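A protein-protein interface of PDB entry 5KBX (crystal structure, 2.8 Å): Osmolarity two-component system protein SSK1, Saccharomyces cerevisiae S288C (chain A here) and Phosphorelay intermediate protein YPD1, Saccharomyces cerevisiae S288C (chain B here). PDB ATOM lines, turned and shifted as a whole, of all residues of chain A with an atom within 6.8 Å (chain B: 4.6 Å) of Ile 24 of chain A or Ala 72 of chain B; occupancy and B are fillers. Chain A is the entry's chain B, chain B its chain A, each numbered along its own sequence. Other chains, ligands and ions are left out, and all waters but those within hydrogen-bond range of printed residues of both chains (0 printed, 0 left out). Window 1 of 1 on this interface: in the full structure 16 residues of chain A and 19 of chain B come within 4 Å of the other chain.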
ATOM      1  N   ILE A  14     -17.435 -33.112  19.328  1.00  0.00           N
ATOM      2  CA  ILE A  14     -18.800 -32.653  19.563  1.00  0.00           C
ATOM      3  C   ILE A  14     -19.057 -31.449  18.668  1.00  0.00           C
ATOM      4  O   ILE A  14     -18.271 -30.492  18.661  1.00  0.00           O
ATOM      5  CB  ILE A  14     -19.038 -32.316  21.045  1.00  0.00           C
ATOM      6  CG1 ILE A  14     -17.831 -31.589  21.633  1.00  0.00           C
ATOM      7  CG2 ILE A  14     -19.319 -33.581  21.839  1.00  0.00           C
ATOM      8  CD1 ILE A  14     -17.935 -31.349  23.123  1.00  0.00           C
ATOM      9  N   GLU A  16     -21.833 -28.662  17.684  1.00  0.00           N
ATOM     10  CA  GLU A  16     -23.065 -27.945  17.984  1.00  0.00           C
ATOM     11  C   GLU A  16     -22.911 -26.493  17.553  1.00  0.00           C
ATOM     12  O   GLU A  16     -21.805 -25.949  17.537  1.00  0.00           O
ATOM     13  CB  GLU A  16     -23.421 -28.021  19.477  1.00  0.00           C
ATOM     14  CG  GLU A  16     -23.569 -29.438  20.010  1.00  0.00           C
ATOM     15  CD  GLU A  16     -23.838 -29.484  21.500  1.00  0.00           C
ATOM     16  OE1 GLU A  16     -25.020 -29.403  21.896  1.00  0.00           O
ATOM     17  OE2 GLU A  16     -22.865 -29.595  22.276  1.00  0.00           O
ATOM     18  N   VAL A  19     -22.048 -22.135  21.381  1.00  0.00           N
ATOM     19  CA  VAL A  19     -20.845 -22.292  22.194  1.00  0.00           C
ATOM     20  C   VAL A  19     -21.198 -22.665  23.628  1.00  0.00           C
ATOM     21  O   VAL A  19     -20.405 -23.316  24.319  1.00  0.00           O
ATOM     22  CB  VAL A  19     -19.990 -21.013  22.140  1.00  0.00           C
ATOM     23  CG1 VAL A  19     -19.470 -20.784  20.730  1.00  0.00           C
ATOM     24  CG2 VAL A  19     -20.793 -19.812  22.615  1.00  0.00           C
ATOM     25  N   ILE A  20     -22.380 -22.265  24.103  1.00  0.00           N
ATOM     26  CA  ILE A  20     -22.801 -22.645  25.447  1.00  0.00           C
ATOM     27  C   ILE A  20     -23.052 -24.146  25.520  1.00  0.00           C
ATOM     28  O   ILE A  20     -22.683 -24.804  26.500  1.00  0.00           O
ATOM     29  CB  ILE A  20     -24.044 -21.839  25.864  1.00  0.00           C
ATOM     30  CG1 ILE A  20     -23.727 -20.343  25.863  1.00  0.00           C
ATOM     31  CG2 ILE A  20     -24.535 -22.279  27.236  1.00  0.00           C
ATOM     32  CD1 ILE A  20     -24.897 -19.477  26.249  1.00  0.00           C
ATOM     33  N   ASN A  21     -23.677 -24.712  24.484  1.00  0.00           N
ATOM     34  CA  ASN A  21     -23.846 -26.159  24.426  1.00  0.00           C
ATOM     35  C   ASN A  21     -22.507 -26.872  24.290  1.00  0.00           C
ATOM     36  O   ASN A  21     -22.344 -27.984  24.805  1.00  0.00           O
ATOM     37  CB  ASN A  21     -24.770 -26.535  23.270  1.00  0.00           C
ATOM     38  CG  ASN A  21     -26.218 -26.180  23.540  1.00  0.00           C
ATOM     39  OD1 ASN A  21     -26.658 -25.064  23.265  1.00  0.00           O
ATOM     40  ND2 ASN A  21     -26.969 -27.134  24.076  1.00  0.00           N
ATOM     41  N   GLN A  22     -21.542 -26.253  23.605  1.00  0.00           N
ATOM     42  CA  GLN A  22     -20.223 -26.864  23.474  1.00  0.00           C
ATOM     43  C   GLN A  22     -19.486 -26.879  24.808  1.00  0.00           C
ATOM     44  O   GLN A  22     -18.749 -27.826  25.106  1.00  0.00           O
ATOM     45  CB  GLN A  22     -19.403 -26.123  22.418  1.00  0.00           C
ATOM     46  CG  GLN A  22     -19.992 -26.178  21.018  1.00  0.00           C
ATOM     47  CD  GLN A  22     -19.210 -25.340  20.023  1.00  0.00           C
ATOM     48  OE1 GLN A  22     -18.197 -24.731  20.366  1.00  0.00           O
ATOM     49  NE2 GLN A  22     -19.681 -25.304  18.782  1.00  0.00           N
ATOM     50  N   ALA A  23     -19.673 -25.838  25.624  1.00  0.00           N
ATOM     51  CA  ALA A  23     -18.994 -25.779  26.913  1.00  0.00           C
ATOM     52  C   ALA A  23     -19.565 -26.787  27.901  1.00  0.00           C
ATOM     53  O   ALA A  23     -18.836 -27.281  28.769  1.00  0.00           O
ATOM     54  CB  ALA A  23     -19.081 -24.365  27.488  1.00  0.00           C
ATOM     55  N   ILE A  24     -20.856 -27.104  27.790  1.00  0.00           N
ATOM     56  CA  ILE A  24     -21.462 -28.077  28.694  1.00  0.00           C
ATOM     57  C   ILE A  24     -20.914 -29.470  28.415  1.00  0.00           C
ATOM     58  O   ILE A  24     -20.449 -30.166  29.326  1.00  0.00           O
ATOM     59  CB  ILE A  24     -22.996 -28.041  28.574  1.00  0.00           C
ATOM     60  CG1 ILE A  24     -23.533 -26.672  28.994  1.00  0.00           C
ATOM     61  CG2 ILE A  24     -23.621 -29.141  29.418  1.00  0.00           C
ATOM     62  CD1 ILE A  24     -25.031 -26.536  28.854  1.00  0.00           C
ATOM     63  N   LEU A  25     -20.960 -29.897  27.152  1.00  0.00           N
ATOM     64  CA  LEU A  25     -20.453 -31.220  26.798  1.00  0.00           C
ATOM     65  C   LEU A  25     -18.941 -31.292  26.961  1.00  0.00           C
ATOM     66  O   LEU A  25     -18.403 -32.331  27.362  1.00  0.00           O
ATOM     67  CB  LEU A  25     -20.861 -31.576  25.368  1.00  0.00           C
ATOM     68  CG  LEU A  25     -22.229 -32.225  25.141  1.00  0.00           C
ATOM     69  CD1 LEU A  25     -23.369 -31.347  25.637  1.00  0.00           C
ATOM     70  CD2 LEU A  25     -22.417 -32.560  23.669  1.00  0.00           C
ATOM     71  N   GLY A  26     -18.237 -30.199  26.654  1.00  0.00           N
ATOM     72  CA  GLY A  26     -16.796 -30.184  26.830  1.00  0.00           C
ATOM     73  C   GLY A  26     -16.370 -30.253  28.282  1.00  0.00           C
ATOM     74  O   GLY A  26     -15.302 -30.787  28.593  1.00  0.00           O
ATOM     75  N   SER A  27     -17.192 -29.719  29.188  1.00  0.00           N
ATOM     76  CA  SER A  27     -16.872 -29.794  30.609  1.00  0.00           C
ATOM     77  C   SER A  27     -16.912 -31.232  31.108  1.00  0.00           C
ATOM     78  O   SER A  27     -16.122 -31.614  31.978  1.00  0.00           O
ATOM     79  CB  SER A  27     -17.840 -28.926  31.412  1.00  0.00           C
ATOM     80  OG  SER A  27     -17.585 -29.034  32.802  1.00  0.00           O
ATOM     81  N   PHE A  28     -17.829 -32.040  30.575  1.00  0.00           N
ATOM     82  CA  PHE A  28     -17.890 -33.441  30.975  1.00  0.00           C
ATOM     83  C   PHE A  28     -16.675 -34.208  30.474  1.00  0.00           C
ATOM     84  O   PHE A  28     -16.109 -35.030  31.202  1.00  0.00           O
ATOM     85  CB  PHE A  28     -19.179 -34.080  30.462  1.00  0.00           C
ATOM     86  CG  PHE A  28     -19.332 -35.520  30.854  1.00  0.00           C
ATOM     87  CD1 PHE A  28     -19.884 -35.859  32.077  1.00  0.00           C
ATOM     88  CD2 PHE A  28     -18.914 -36.532  30.007  1.00  0.00           C
ATOM     89  CE1 PHE A  28     -20.019 -37.181  32.444  1.00  0.00           C
ATOM     90  CE2 PHE A  28     -19.046 -37.854  30.370  1.00  0.00           C
ATOM     91  CZ  PHE A  28     -19.597 -38.178  31.591  1.00  0.00           C
ATOM     92  N   LEU A  29     -16.262 -33.957  29.230  1.00  0.00           N
ATOM     93  CA  LEU A  29     -15.092 -34.640  28.688  1.00  0.00           C
ATOM     94  C   LEU A  29     -13.818 -34.190  29.391  1.00  0.00           C
ATOM     95  O   LEU A  29     -12.924 -35.004  29.650  1.00  0.00           O
ATOM     96  CB  LEU A  29     -14.995 -34.397  27.184  1.00  0.00           C
ATOM     97  CG  LEU A  29     -16.226 -34.802  26.369  1.00  0.00           C
ATOM     98  CD1 LEU A  29     -16.003 -34.566  24.887  1.00  0.00           C
ATOM     99  CD2 LEU A  29     -16.574 -36.253  26.629  1.00  0.00           C
ATOM    100  N   PRO A 139     -32.431 -31.364  24.870  1.00  0.00           N
ATOM    101  CA  PRO A 139     -31.072 -31.088  25.354  1.00  0.00           C
ATOM    102  C   PRO A 139     -30.333 -32.340  25.817  1.00  0.00           C
ATOM    103  O   PRO A 139     -30.932 -33.208  26.447  1.00  0.00           O
ATOM    104  CB  PRO A 139     -31.306 -30.127  26.522  1.00  0.00           C
ATOM    105  CG  PRO A 139     -32.678 -30.444  26.995  1.00  0.00           C
ATOM    106  CD  PRO A 139     -33.454 -30.781  25.756  1.00  0.00           C
ATOM    107  N   VAL A 140     -29.042 -32.419  25.490  1.00  0.00           N
ATOM    108  CA  VAL A 140     -28.278 -33.631  25.752  1.00  0.00           C
ATOM    109  C   VAL A 140     -28.223 -33.892  27.248  1.00  0.00           C
ATOM    110  O   VAL A 140     -27.889 -33.005  28.042  1.00  0.00           O
ATOM    111  CB  VAL A 140     -26.872 -33.521  25.145  1.00  0.00           C
ATOM    112  CG1 VAL A 140     -26.040 -34.739  25.497  1.00  0.00           C
ATOM    113  CG2 VAL A 140     -26.967 -33.362  23.640  1.00  0.00           C
ATOM    114  N   LEU A 142     -26.472 -35.379  30.342  1.00  0.00           N
ATOM    115  CA  LEU A 142     -25.086 -35.706  30.662  1.00  0.00           C
ATOM    116  C   LEU A 142     -24.939 -37.145  31.137  1.00  0.00           C
ATOM    117  O   LEU A 142     -23.912 -37.780  30.874  1.00  0.00           O
ATOM    118  CB  LEU A 142     -24.544 -34.737  31.712  1.00  0.00           C
ATOM    119  CG  LEU A 142     -24.324 -33.296  31.242  1.00  0.00           C
ATOM    120  CD1 LEU A 142     -23.709 -32.457  32.350  1.00  0.00           C
ATOM    121  CD2 LEU A 142     -23.454 -33.268  29.997  1.00  0.00           C
ATOM    122  N   LEU A 145     -25.164 -38.930  27.944  1.00  0.00           N
ATOM    123  CA  LEU A 145     -23.918 -38.702  27.220  1.00  0.00           C
ATOM    124  C   LEU A 145     -22.811 -39.605  27.746  1.00  0.00           C
ATOM    125  O   LEU A 145     -21.996 -40.119  26.970  1.00  0.00           O
ATOM    126  CB  LEU A 145     -23.509 -37.232  27.331  1.00  0.00           C
ATOM    127  CG  LEU A 145     -22.178 -36.829  26.693  1.00  0.00           C
ATOM    128  CD1 LEU A 145     -22.271 -36.873  25.179  1.00  0.00           C
ATOM    129  CD2 LEU A 145     -21.741 -35.450  27.167  1.00  0.00           C
ATOM    130  N   ILE B  13     -31.883 -30.869  34.996  1.00  0.00           N
ATOM    131  CA  ILE B  13     -30.896 -30.619  33.952  1.00  0.00           C
ATOM    132  C   ILE B  13     -29.756 -29.756  34.479  1.00  0.00           C
ATOM    133  O   ILE B  13     -28.593 -29.951  34.109  1.00  0.00           O
ATOM    134  CB  ILE B  13     -31.577 -29.978  32.727  1.00  0.00           C
ATOM    135  CG1 ILE B  13     -32.542 -30.968  32.070  1.00  0.00           C
ATOM    136  CG2 ILE B  13     -30.544 -29.496  31.719  1.00  0.00           C
ATOM    137  CD1 ILE B  13     -33.156 -30.455  30.782  1.00  0.00           C
ATOM    138  N   ILE B  17     -25.087 -29.968  35.745  1.00  0.00           N
ATOM    139  CA  ILE B  17     -24.103 -28.977  35.324  1.00  0.00           C
ATOM    140  C   ILE B  17     -23.411 -28.369  36.537  1.00  0.00           C
ATOM    141  O   ILE B  17     -22.201 -28.119  36.518  1.00  0.00           O
ATOM    142  CB  ILE B  17     -24.772 -27.900  34.452  1.00  0.00           C
ATOM    143  CG1 ILE B  17     -25.406 -28.536  33.213  1.00  0.00           C
ATOM    144  CG2 ILE B  17     -23.765 -26.833  34.048  1.00  0.00           C
ATOM    145  CD1 ILE B  17     -26.076 -27.540  32.299  1.00  0.00           C
ATOM    146  N   MET B  20     -20.511 -30.289  38.155  1.00  0.00           N
ATOM    147  CA  MET B  20     -19.171 -30.123  37.611  1.00  0.00           C
ATOM    148  C   MET B  20     -18.476 -28.874  38.138  1.00  0.00           C
ATOM    149  O   MET B  20     -17.422 -28.497  37.615  1.00  0.00           O
ATOM    150  CB  MET B  20     -19.223 -30.093  36.082  1.00  0.00           C
ATOM    151  CG  MET B  20     -19.739 -31.380  35.458  1.00  0.00           C
ATOM    152  SD  MET B  20     -19.738 -31.345  33.655  1.00  0.00           S
ATOM    153  CE  MET B  20     -20.844 -29.971  33.342  1.00  0.00           C
ATOM    154  N   LEU B  31     -21.382 -20.084  32.902  1.00  0.00           N
ATOM    155  CA  LEU B  31     -22.320 -20.378  31.823  1.00  0.00           C
ATOM    156  C   LEU B  31     -23.558 -19.494  31.911  1.00  0.00           C
ATOM    157  O   LEU B  31     -24.070 -19.032  30.885  1.00  0.00           O
ATOM    158  CB  LEU B  31     -22.717 -21.853  31.853  1.00  0.00           C
ATOM    159  CG  LEU B  31     -21.653 -22.878  31.463  1.00  0.00           C
ATOM    160  CD1 LEU B  31     -22.219 -24.285  31.555  1.00  0.00           C
ATOM    161  CD2 LEU B  31     -21.132 -22.598  30.063  1.00  0.00           C
ATOM    162  N   GLY B  68     -31.710 -23.799  22.115  1.00  0.00           N
ATOM    163  CA  GLY B  68     -30.757 -24.856  22.407  1.00  0.00           C
ATOM    164  C   GLY B  68     -29.924 -24.597  23.647  1.00  0.00           C
ATOM    165  O   GLY B  68     -29.531 -25.540  24.340  1.00  0.00           O
ATOM    166  N   SER B  69     -29.645 -23.327  23.946  1.00  0.00           N
ATOM    167  CA  SER B  69     -28.845 -23.002  25.121  1.00  0.00           C
ATOM    168  C   SER B  69     -29.704 -22.942  26.378  1.00  0.00           C
ATOM    169  O   SER B  69     -29.321 -23.474  27.427  1.00  0.00           O
ATOM    170  CB  SER B  69     -28.112 -21.676  24.910  1.00  0.00           C
ATOM    171  OG  SER B  69     -29.025 -20.621  24.664  1.00  0.00           O
ATOM    172  N   SER B  70     -30.869 -22.296  26.290  1.00  0.00           N
ATOM    173  CA  SER B  70     -31.742 -22.183  27.453  1.00  0.00           C
ATOM    174  C   SER B  70     -32.284 -23.538  27.885  1.00  0.00           C
ATOM    175  O   SER B  70     -32.505 -23.763  29.081  1.00  0.00           O
ATOM    176  CB  SER B  70     -32.891 -21.219  27.157  1.00  0.00           C
ATOM    177  OG  SER B  70     -33.623 -21.634  26.016  1.00  0.00           O
ATOM    178  N   ALA B  71     -32.504 -24.453  26.937  1.00  0.00           N
ATOM    179  CA  ALA B  71     -32.981 -25.783  27.301  1.00  0.00           C
ATOM    180  C   ALA B  71     -31.876 -26.604  27.955  1.00  0.00           C
ATOM    181  O   ALA B  71     -32.132 -27.355  28.904  1.00  0.00           O
ATOM    182  CB  ALA B  71     -33.529 -26.503  26.070  1.00  0.00           C
ATOM    183  N   ALA B  72     -30.642 -26.474  27.462  1.00  0.00           N
ATOM    184  CA  ALA B  72     -29.526 -27.214  28.038  1.00  0.00           C
ATOM    185  C   ALA B  72     -29.164 -26.725  29.433  1.00  0.00           C
ATOM    186  O   ALA B  72     -28.531 -27.468  30.190  1.00  0.00           O
ATOM    187  CB  ALA B  72     -28.304 -27.122  27.124  1.00  0.00           C
ATOM    188  N   LEU B  73     -29.546 -25.499  29.788  1.00  0.00           N
ATOM    189  CA  LEU B  73     -29.307 -24.955  31.116  1.00  0.00           C
ATOM    190  C   LEU B  73     -30.501 -25.130  32.043  1.00  0.00           C
ATOM    191  O   LEU B  73     -30.481 -24.615  33.167  1.00  0.00           O
ATOM    192  CB  LEU B  73     -28.932 -23.474  31.021  1.00  0.00           C
ATOM    193  CG  LEU B  73     -27.596 -23.150  30.349  1.00  0.00           C
ATOM    194  CD1 LEU B  73     -27.381 -21.647  30.286  1.00  0.00           C
ATOM    195  CD2 LEU B  73     -26.449 -23.825  31.085  1.00  0.00           C
ATOM    196  N   GLY B  74     -31.537 -25.840  31.603  1.00  0.00           N
ATOM    197  CA  GLY B  74     -32.708 -26.063  32.425  1.00  0.00           C
ATOM    198  C   GLY B  74     -33.698 -24.922  32.460  1.00  0.00           C
ATOM    199  O   GLY B  74     -34.657 -24.981  33.238  1.00  0.00           O
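SD of Met 20 of chain B sits at hydrogen-bond distance from OG of Ser 27 of chain A, at 3.3 Å.
SD of Met 20 of chain B lies within hydrogen-bond range of N of Phe 28 of chain A (3.7 Å).
O of Gly 68 of chain B sits at hydrogen-bond distance from ND2 of Asn 21 of chain A (3.0 Å).
Asn 21 of chain A touches Ser 69 of chain B.
Ala 72 of chain B touches Asn 21 of chain A (CB to ND2, 3.3 Å).
CD2 of Leu 31 of chain B touches CB of Ala 23 of chain A, at 3.7 Å.
CD1 of Ile 24 of chain A touches CD1 of Ile 17 of chain B, 3.7 Å away.
CB of Ala 72 of chain B touches CD1 of Ile 24 of chain A, at 3.7 Å.
Leu 73 of chain B touches Ile 24 of chain A.
Pro 139 of chain A touches Ile 13 of chain B (CG to CD1, 3.8 Å).
Ala 71 of chain B touches Pro 139 of chain A (O to CG, 3.7 Å).
Ala 72 of chain B touches Pro 139 of chain A.
CE of Met 20 of chain B touches CD1 of Leu 142 of chain A, at 3.9 Å.
Of chain B, only Ile 17 (3.7 Å), Leu 31 (3.7 Å), Ala 72 (3.7 Å) and Leu 73 (3.8 Å) come within 4 Å of Ile 24 of chain A.
Ala 72 of chain B touches just these residues of chain A: Asn 21, Ile 24 and Pro 139.
Of the printed residues of chain A, Leu 31 of chain B touches Ala 23 (3.7 Å) and Ile 24 (3.7 Å).
Printed residues of chain A within 4 Å of Gly 68 of chain B: Asn 21 (3.0 Å).
Val 19 of chain A touches none of the printed residues of chain B.
Gly 74 of chain B touches none of the printed residues of chain A.
The nearest residue of chain B that does not touch Ile 24 of chain A is Met 20 of chain B (4.04 Å).
The nearest residue of chain A that does not touch Ala 72 of chain B is Val 140 of chain A (5.6 Å).
Of the 11 printed residues of chain B, 9 touch a printed residue of chain A.
Hydrophobic or aromatic side chains of chain B within 4 Å of the printed part of chain A: Ile 13, Ile 17, Met 20, Leu 31, Ala 72 and Leu 73.
Printed residues of chain A that touch a printed residue of chain B: Asn 21, Ala 23, Ile 24, Ser 27, Phe 28, Pro 139 and Leu 142.
Hydrophobic or aromatic side chains of chain A within 4 Å of the printed part of chain B: Ala 23, Ile 24, Pro 139 and Leu 142.
Among the printed residues, 14 pairs touch across the chains.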
